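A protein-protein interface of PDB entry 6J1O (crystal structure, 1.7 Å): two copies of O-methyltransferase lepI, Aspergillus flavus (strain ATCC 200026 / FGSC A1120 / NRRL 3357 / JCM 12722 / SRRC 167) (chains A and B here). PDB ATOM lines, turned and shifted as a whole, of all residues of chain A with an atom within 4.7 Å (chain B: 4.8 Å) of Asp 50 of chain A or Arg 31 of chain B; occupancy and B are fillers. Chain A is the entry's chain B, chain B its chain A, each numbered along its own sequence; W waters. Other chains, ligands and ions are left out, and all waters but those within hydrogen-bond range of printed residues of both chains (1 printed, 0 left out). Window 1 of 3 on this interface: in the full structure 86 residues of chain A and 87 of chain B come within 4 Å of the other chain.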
ATOM      1  N   GLN A  34      -4.207   5.217  21.012  1.00  0.00           N
ATOM      2  CA  GLN A  34      -3.070   4.814  20.194  1.00  0.00           C
ATOM      3  C   GLN A  34      -3.378   3.540  19.415  1.00  0.00           C
ATOM      4  O   GLN A  34      -3.175   3.479  18.198  1.00  0.00           O
ATOM      5  CB  GLN A  34      -1.841   4.616  21.081  1.00  0.00           C
ATOM      6  CG  GLN A  34      -0.629   4.109  20.335  1.00  0.00           C
ATOM      7  CD  GLN A  34       0.407   3.506  21.264  1.00  0.00           C
ATOM      8  OE1 GLN A  34       1.216   2.674  20.849  1.00  0.00           O
ATOM      9  NE2 GLN A  34       0.387   3.923  22.527  1.00  0.00           N
ATOM     10  N   MET A  45       4.706  -3.146  13.660  1.00  0.00           N
ATOM     11  CA  MET A  45       5.966  -2.523  14.065  1.00  0.00           C
ATOM     12  C   MET A  45       6.029  -2.326  15.575  1.00  0.00           C
ATOM     13  O   MET A  45       7.085  -2.509  16.190  1.00  0.00           O
ATOM     14  CB  MET A  45       6.145  -1.187  13.345  1.00  0.00           C
ATOM     15  CG  MET A  45       6.512  -1.338  11.889  1.00  0.00           C
ATOM     16  SD  MET A  45       8.172  -2.016  11.676  1.00  0.00           S
ATOM     17  CE  MET A  45       9.162  -0.659  12.283  1.00  0.00           C
ATOM     18  N   ARG A  46       4.911  -1.923  16.184  1.00  0.00           N
ATOM     19  CA  ARG A  46       4.870  -1.715  17.627  1.00  0.00           C
ATOM     20  C   ARG A  46       5.120  -3.019  18.364  1.00  0.00           C
ATOM     21  O   ARG A  46       5.928  -3.078  19.300  1.00  0.00           O
ATOM     22  CB  ARG A  46       3.520  -1.110  18.026  1.00  0.00           C
ATOM     23  CG  ARG A  46       3.217  -1.191  19.512  1.00  0.00           C
ATOM     24  CD  ARG A  46       1.911  -0.497  19.870  1.00  0.00           C
ATOM     25  NE  ARG A  46       0.719  -1.162  19.346  1.00  0.00           N
ATOM     26  CZ  ARG A  46       0.199  -2.282  19.847  1.00  0.00           C
ATOM     27  NH1 ARG A  46       0.778  -2.888  20.882  1.00  0.00           N
ATOM     28  NH2 ARG A  46      -0.896  -2.797  19.306  1.00  0.00           N
ATOM     29  N   MET A  47       4.424  -4.084  17.960  1.00  0.00           N
ATOM     30  CA  MET A  47       4.661  -5.380  18.586  1.00  0.00           C
ATOM     31  C   MET A  47       6.090  -5.857  18.348  1.00  0.00           C
ATOM     32  O   MET A  47       6.701  -6.478  19.227  1.00  0.00           O
ATOM     33  CB  MET A  47       3.650  -6.404  18.069  1.00  0.00           C
ATOM     34  CG  MET A  47       2.248  -6.174  18.596  1.00  0.00           C
ATOM     35  SD  MET A  47       1.078  -7.413  18.021  1.00  0.00           S
ATOM     36  CE  MET A  47      -0.446  -6.736  18.671  1.00  0.00           C
ATOM     37  N   SER A  48       6.644  -5.553  17.176  1.00  0.00           N
ATOM     38  CA  SER A  48       7.992  -6.004  16.845  1.00  0.00           C
ATOM     39  C   SER A  48       9.048  -5.285  17.677  1.00  0.00           C
ATOM     40  O   SER A  48      10.056  -5.887  18.059  1.00  0.00           O
ATOM     41  CB  SER A  48       8.271  -5.785  15.359  1.00  0.00           C
ATOM     42  OG  SER A  48       7.412  -6.565  14.541  1.00  0.00           O
ATOM     43  N   LEU A  49       8.849  -3.991  17.943  1.00  0.00           N
ATOM     44  CA  LEU A  49       9.910  -3.143  18.467  1.00  0.00           C
ATOM     45  C   LEU A  49       9.770  -2.748  19.930  1.00  0.00           C
ATOM     46  O   LEU A  49      10.783  -2.417  20.549  1.00  0.00           O
ATOM     47  CB  LEU A  49      10.014  -1.855  17.632  1.00  0.00           C
ATOM     48  CG  LEU A  49      10.394  -2.000  16.157  1.00  0.00           C
ATOM     49  CD1 LEU A  49      10.530  -0.627  15.537  1.00  0.00           C
ATOM     50  CD2 LEU A  49      11.682  -2.803  15.975  1.00  0.00           C
ATOM     51  N   ASP A  50       8.564  -2.744  20.501  1.00  0.00           N
ATOM     52  CA  ASP A  50       8.461  -2.318  21.895  1.00  0.00           C
ATOM     53  C   ASP A  50       9.201  -3.280  22.809  1.00  0.00           C
ATOM     54  O   ASP A  50       9.605  -2.897  23.915  1.00  0.00           O
ATOM     55  CB  ASP A  50       6.990  -2.199  22.310  1.00  0.00           C
ATOM     56  CG  ASP A  50       6.330  -0.927  21.785  1.00  0.00           C
ATOM     57  OD1 ASP A  50       6.988  -0.157  21.055  1.00  0.00           O
ATOM     58  OD2 ASP A  50       5.147  -0.696  22.106  1.00  0.00           O
ATOM     59  N   THR A  51       9.408  -4.507  22.330  1.00  0.00           N
ATOM     60  CA  THR A  51      10.259  -5.500  22.970  1.00  0.00           C
ATOM     61  C   THR A  51      11.662  -4.968  23.265  1.00  0.00           C
ATOM     62  O   THR A  51      12.293  -5.350  24.267  1.00  0.00           O
ATOM     63  CB  THR A  51      10.348  -6.702  22.033  1.00  0.00           C
ATOM     64  OG1 THR A  51       9.034  -7.068  21.583  1.00  0.00           O
ATOM     65  CG2 THR A  51      10.925  -7.822  22.735  1.00  0.00           C
ATOM     66  N   CYS A  52      12.173  -4.105  22.386  1.00  0.00           N
ATOM     67  CA  CYS A  52      13.522  -3.568  22.531  1.00  0.00           C
ATOM     68  C   CYS A  52      13.711  -2.847  23.852  1.00  0.00           C
ATOM     69  O   CYS A  52      14.842  -2.748  24.340  1.00  0.00           O
ATOM     70  CB  CYS A  52      13.838  -2.590  21.403  1.00  0.00           C
ATOM     71  SG  CYS A  52      14.007  -3.317  19.768  1.00  0.00           S
ATOM     72  N   GLN A  53      12.637  -2.294  24.422  1.00  0.00           N
ATOM     73  CA  GLN A  53      12.801  -1.446  25.602  1.00  0.00           C
ATOM     74  C   GLN A  53      13.372  -2.224  26.776  1.00  0.00           C
ATOM     75  O   GLN A  53      14.228  -1.711  27.505  1.00  0.00           O
ATOM     76  CB  GLN A  53      11.477  -0.802  25.997  1.00  0.00           C
ATOM     77  CG  GLN A  53      10.953   0.162  24.955  1.00  0.00           C
ATOM     78  CD  GLN A  53       9.874   1.067  25.484  1.00  0.00           C
ATOM     79  OE1 GLN A  53       9.863   1.420  26.660  1.00  0.00           O
ATOM     80  NE2 GLN A  53       8.959   1.462  24.611  1.00  0.00           N
ATOM     81  N   VAL A  54      12.905  -3.457  26.990  1.00  0.00           N
ATOM     82  CA  VAL A  54      13.404  -4.231  28.127  1.00  0.00           C
ATOM     83  C   VAL A  54      14.865  -4.618  27.921  1.00  0.00           C
ATOM     84  O   VAL A  54      15.672  -4.556  28.858  1.00  0.00           O
ATOM     85  CB  VAL A  54      12.520  -5.466  28.369  1.00  0.00           C
ATOM     86  CG1 VAL A  54      13.055  -6.293  29.539  1.00  0.00           C
ATOM     87  CG2 VAL A  54      11.095  -5.043  28.622  1.00  0.00           C
ATOM     88  N   ASN B  27      -0.344   9.940  16.986  1.00  0.00           N
ATOM     89  CA  ASN B  27      -0.079   8.714  17.738  1.00  0.00           C
ATOM     90  C   ASN B  27       1.250   8.785  18.484  1.00  0.00           C
ATOM     91  O   ASN B  27       1.342   8.351  19.642  1.00  0.00           O
ATOM     92  CB  ASN B  27      -0.111   7.501  16.815  1.00  0.00           C
ATOM     93  CG  ASN B  27      -1.391   6.704  16.965  1.00  0.00           C
ATOM     94  OD1 ASN B  27      -2.425   7.253  17.344  1.00  0.00           O
ATOM     95  ND2 ASN B  27      -1.323   5.403  16.701  1.00  0.00           N
ATOM     96  N   ASP B  28       2.296   9.314  17.838  1.00  0.00           N
ATOM     97  CA  ASP B  28       3.563   9.469  18.551  1.00  0.00           C
ATOM     98  C   ASP B  28       3.404  10.393  19.753  1.00  0.00           C
ATOM     99  O   ASP B  28       3.998  10.156  20.818  1.00  0.00           O
ATOM    100  CB  ASP B  28       4.651   9.992  17.609  1.00  0.00           C
ATOM    101  CG  ASP B  28       5.305   8.884  16.787  1.00  0.00           C
ATOM    102  OD1 ASP B  28       4.854   7.722  16.880  1.00  0.00           O
ATOM    103  OD2 ASP B  28       6.274   9.176  16.045  1.00  0.00           O
ATOM    104  N   ALA B  29       2.599  11.452  19.603  1.00  0.00           N
ATOM    105  CA  ALA B  29       2.348  12.355  20.724  1.00  0.00           C
ATOM    106  C   ALA B  29       1.625  11.648  21.862  1.00  0.00           C
ATOM    107  O   ALA B  29       1.921  11.889  23.039  1.00  0.00           O
ATOM    108  CB  ALA B  29       1.541  13.564  20.254  1.00  0.00           C
ATOM    109  N   LEU B  30       0.670  10.774  21.536  1.00  0.00           N
ATOM    110  CA  LEU B  30      -0.032  10.029  22.577  1.00  0.00           C
ATOM    111  C   LEU B  30       0.929   9.124  23.335  1.00  0.00           C
ATOM    112  O   LEU B  30       0.820   8.973  24.562  1.00  0.00           O
ATOM    113  CB  LEU B  30      -1.165   9.204  21.959  1.00  0.00           C
ATOM    114  CG  LEU B  30      -2.281   9.976  21.247  1.00  0.00           C
ATOM    115  CD1 LEU B  30      -3.268   9.028  20.588  1.00  0.00           C
ATOM    116  CD2 LEU B  30      -2.984  10.886  22.235  1.00  0.00           C
ATOM    117  N   ARG B  31       1.873   8.506  22.619  1.00  0.00           N
ATOM    118  CA  ARG B  31       2.872   7.671  23.285  1.00  0.00           C
ATOM    119  C   ARG B  31       3.753   8.499  24.218  1.00  0.00           C
ATOM    120  O   ARG B  31       3.979   8.125  25.379  1.00  0.00           O
ATOM    121  CB  ARG B  31       3.702   6.942  22.231  1.00  0.00           C
ATOM    122  CG  ARG B  31       4.724   5.966  22.770  1.00  0.00           C
ATOM    123  CD  ARG B  31       5.497   5.345  21.612  1.00  0.00           C
ATOM    124  NE  ARG B  31       4.624   4.578  20.721  1.00  0.00           N
ATOM    125  CZ  ARG B  31       4.753   3.278  20.466  1.00  0.00           C
ATOM    126  NH1 ARG B  31       3.905   2.674  19.639  1.00  0.00           N
ATOM    127  NH2 ARG B  31       5.731   2.582  21.028  1.00  0.00           N
ATOM    128  N   GLU B  32       4.255   9.637  23.730  1.00  0.00           N
ATOM    129  CA  GLU B  32       5.069  10.511  24.574  1.00  0.00           C
ATOM    130  C   GLU B  32       4.305  10.965  25.817  1.00  0.00           C
ATOM    131  O   GLU B  32       4.868  11.013  26.920  1.00  0.00           O
ATOM    132  CB  GLU B  32       5.540  11.721  23.765  1.00  0.00           C
ATOM    133  CG  GLU B  32       6.391  12.686  24.566  1.00  0.00           C
ATOM    134  CD  GLU B  32       6.655  13.986  23.831  1.00  0.00           C
ATOM    135  OE1 GLU B  32       6.594  13.983  22.583  1.00  0.00           O
ATOM    136  OE2 GLU B  32       6.914  15.010  24.500  1.00  0.00           O
ATOM    137  N   LEU B  33       3.021  11.298  25.661  1.00  0.00           N
ATOM    138  CA  LEU B  33       2.215  11.699  26.813  1.00  0.00           C
ATOM    139  C   LEU B  33       2.092  10.561  27.812  1.00  0.00           C
ATOM    140  O   LEU B  33       2.250  10.758  29.026  1.00  0.00           O
ATOM    141  CB  LEU B  33       0.831  12.151  26.351  1.00  0.00           C
ATOM    142  CG  LEU B  33       0.809  13.553  25.748  1.00  0.00           C
ATOM    143  CD1 LEU B  33      -0.481  13.785  24.977  1.00  0.00           C
ATOM    144  CD2 LEU B  33       0.978  14.572  26.869  1.00  0.00           C
ATOM    145  N   GLN B  34       1.794   9.358  27.317  1.00  0.00           N
ATOM    146  CA  GLN B  34       1.721   8.191  28.191  1.00  0.00           C
ATOM    147  C   GLN B  34       2.994   8.037  29.008  1.00  0.00           C
ATOM    148  O   GLN B  34       2.943   7.889  30.237  1.00  0.00           O
ATOM    149  CB  GLN B  34       1.468   6.929  27.370  1.00  0.00           C
ATOM    150  CG  GLN B  34       0.008   6.614  27.152  1.00  0.00           C
ATOM    151  CD  GLN B  34      -0.181   5.463  26.197  1.00  0.00           C
ATOM    152  OE1 GLN B  34      -0.405   5.669  25.010  1.00  0.00           O
ATOM    153  NE2 GLN B  34      -0.072   4.243  26.703  1.00  0.00           N
ATOM    154  N   TYR B  35       4.150   8.077  28.340  1.00  0.00           N
ATOM    155  CA  TYR B  35       5.412   7.865  29.047  1.00  0.00           C
ATOM    156  C   TYR B  35       5.688   8.975  30.052  1.00  0.00           C
ATOM    157  O   TYR B  35       6.255   8.724  31.123  1.00  0.00           O
ATOM    158  CB  TYR B  35       6.576   7.767  28.061  1.00  0.00           C
ATOM    159  CG  TYR B  35       6.552   6.570  27.139  1.00  0.00           C
ATOM    160  CD1 TYR B  35       5.637   5.534  27.313  1.00  0.00           C
ATOM    161  CD2 TYR B  35       7.472   6.462  26.103  1.00  0.00           C
ATOM    162  CE1 TYR B  35       5.628   4.434  26.460  1.00  0.00           C
ATOM    163  CE2 TYR B  35       7.474   5.372  25.253  1.00  0.00           C
ATOM    164  CZ  TYR B  35       6.560   4.357  25.438  1.00  0.00           C
ATOM    165  OH  TYR B  35       6.583   3.281  24.576  1.00  0.00           O
ATOM    166  N   TRP B 333      10.840   6.248  17.406  1.00  0.00           N
ATOM    167  CA  TRP B 333      11.084   4.893  17.904  1.00  0.00           C
ATOM    168  C   TRP B 333      11.066   3.859  16.785  1.00  0.00           C
ATOM    169  O   TRP B 333      11.786   2.855  16.858  1.00  0.00           O
ATOM    170  CB  TRP B 333      10.060   4.525  18.989  1.00  0.00           C
ATOM    171  CG  TRP B 333       8.641   4.479  18.495  1.00  0.00           C
ATOM    172  CD1 TRP B 333       7.728   5.500  18.516  1.00  0.00           C
ATOM    173  CD2 TRP B 333       7.976   3.361  17.889  1.00  0.00           C
ATOM    174  NE1 TRP B 333       6.541   5.084  17.958  1.00  0.00           N
ATOM    175  CE2 TRP B 333       6.667   3.776  17.567  1.00  0.00           C
ATOM    176  CE3 TRP B 333       8.362   2.051  17.584  1.00  0.00           C
ATOM    177  CZ2 TRP B 333       5.740   2.924  16.955  1.00  0.00           C
ATOM    178  CZ3 TRP B 333       7.436   1.208  16.966  1.00  0.00           C
ATOM    179  CH2 TRP B 333       6.146   1.649  16.665  1.00  0.00           C
HETATM  180  O   HOH W   1       3.159   1.060  22.491  1.00  0.00           O
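Of the 11 printed residues of chain A, 6 touch a printed residue of chain B. Among the printed residues, 10 pairs touch across the chains. Among the printed residues, Asp or Glu carboxylates within 4 Å of a Lys or Arg side-chain nitrogen of the other chain: Asp 50 of chain A with Arg 31 of chain B (3.0 Å).
Of the printed residues of chain B, Arg 46 of chain A touches Arg 31 and Trp 333. Of the printed residues of chain B, Leu 49 of chain A touches Trp 333. Asp 50 of chain A touches one residue of chain B. Thr 51 of chain A touches none of the printed residues of chain B. Of the printed residues of chain A, Asn 27 of chain B touches Gln 34. Ala 29 of chain B touches none of the printed residues of chain A. Of the printed residues of chain A, Arg 31 of chain B touches Gln 34 (2.9 Å), Arg 46 (3.8 Å) and Asp 50 (3.0 Å).
NH2 of Arg 31 of chain B is in salt-bridge range of OD1 of Asp 50 of chain A. OE1 of Gln 34 of chain A lies within hydrogen-bond range of NH1 of Arg 31 of chain B (2.9 Å). The side-chain amide nitrogen (NE2) of Gln 34 of chain A sits at hydrogen-bond distance from the side-chain amide oxygen (OE1) of Gln 34 of chain B, 3.1 Å away. The backbone carbonyl oxygen of Gln 34 of chain A lies within hydrogen-bond range of the side-chain amide nitrogen of Asn 27 of chain B. The side-chain amide nitrogen (NE2) of Gln 53 of chain A sits at hydrogen-bond distance from the side-chain hydroxyl (OH) of Tyr 35 of chain B, 3.0 Å away.
Gln 34 of chain A touches its own counterpart, Gln 34 of chain B. 1 position is printed for both chains. Of the 10 pairs that touch across the chains among the printed residues, 1 has its exchanged pair printed and touching as well.
NE1 of Trp 333 of chain B is in hydrogen-bond range of OD1 of Asp 28 of chain B (3.3 Å). SG of Cys 52 of chain A lies close to O of Leu 49 of chain A, 3.4 Å away.
N of Gln 34 of chain A touches CD1 of Leu 30 of chain B (3.9 Å). Met 45 of chain A touches Trp 333 of chain B (O to CZ3, 3.8 Å). CD of Arg 46 of chain A touches NH1 of Arg 31 of chain B, 3.8 Å away. Arg 46 of chain A touches Trp 333 of chain B (CA to CH2, 3.7 Å). CZ3 of Trp 333 of chain B touches CD1 of Leu 49 of chain A (3.9 Å).
Water W1 lies within hydrogen-bond range of the side-chain carboxylate of Asp 50 of chain A, the side-chain amide oxygen of Gln 34 of chain A and the guanidinium group of Arg 31 of chain B.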
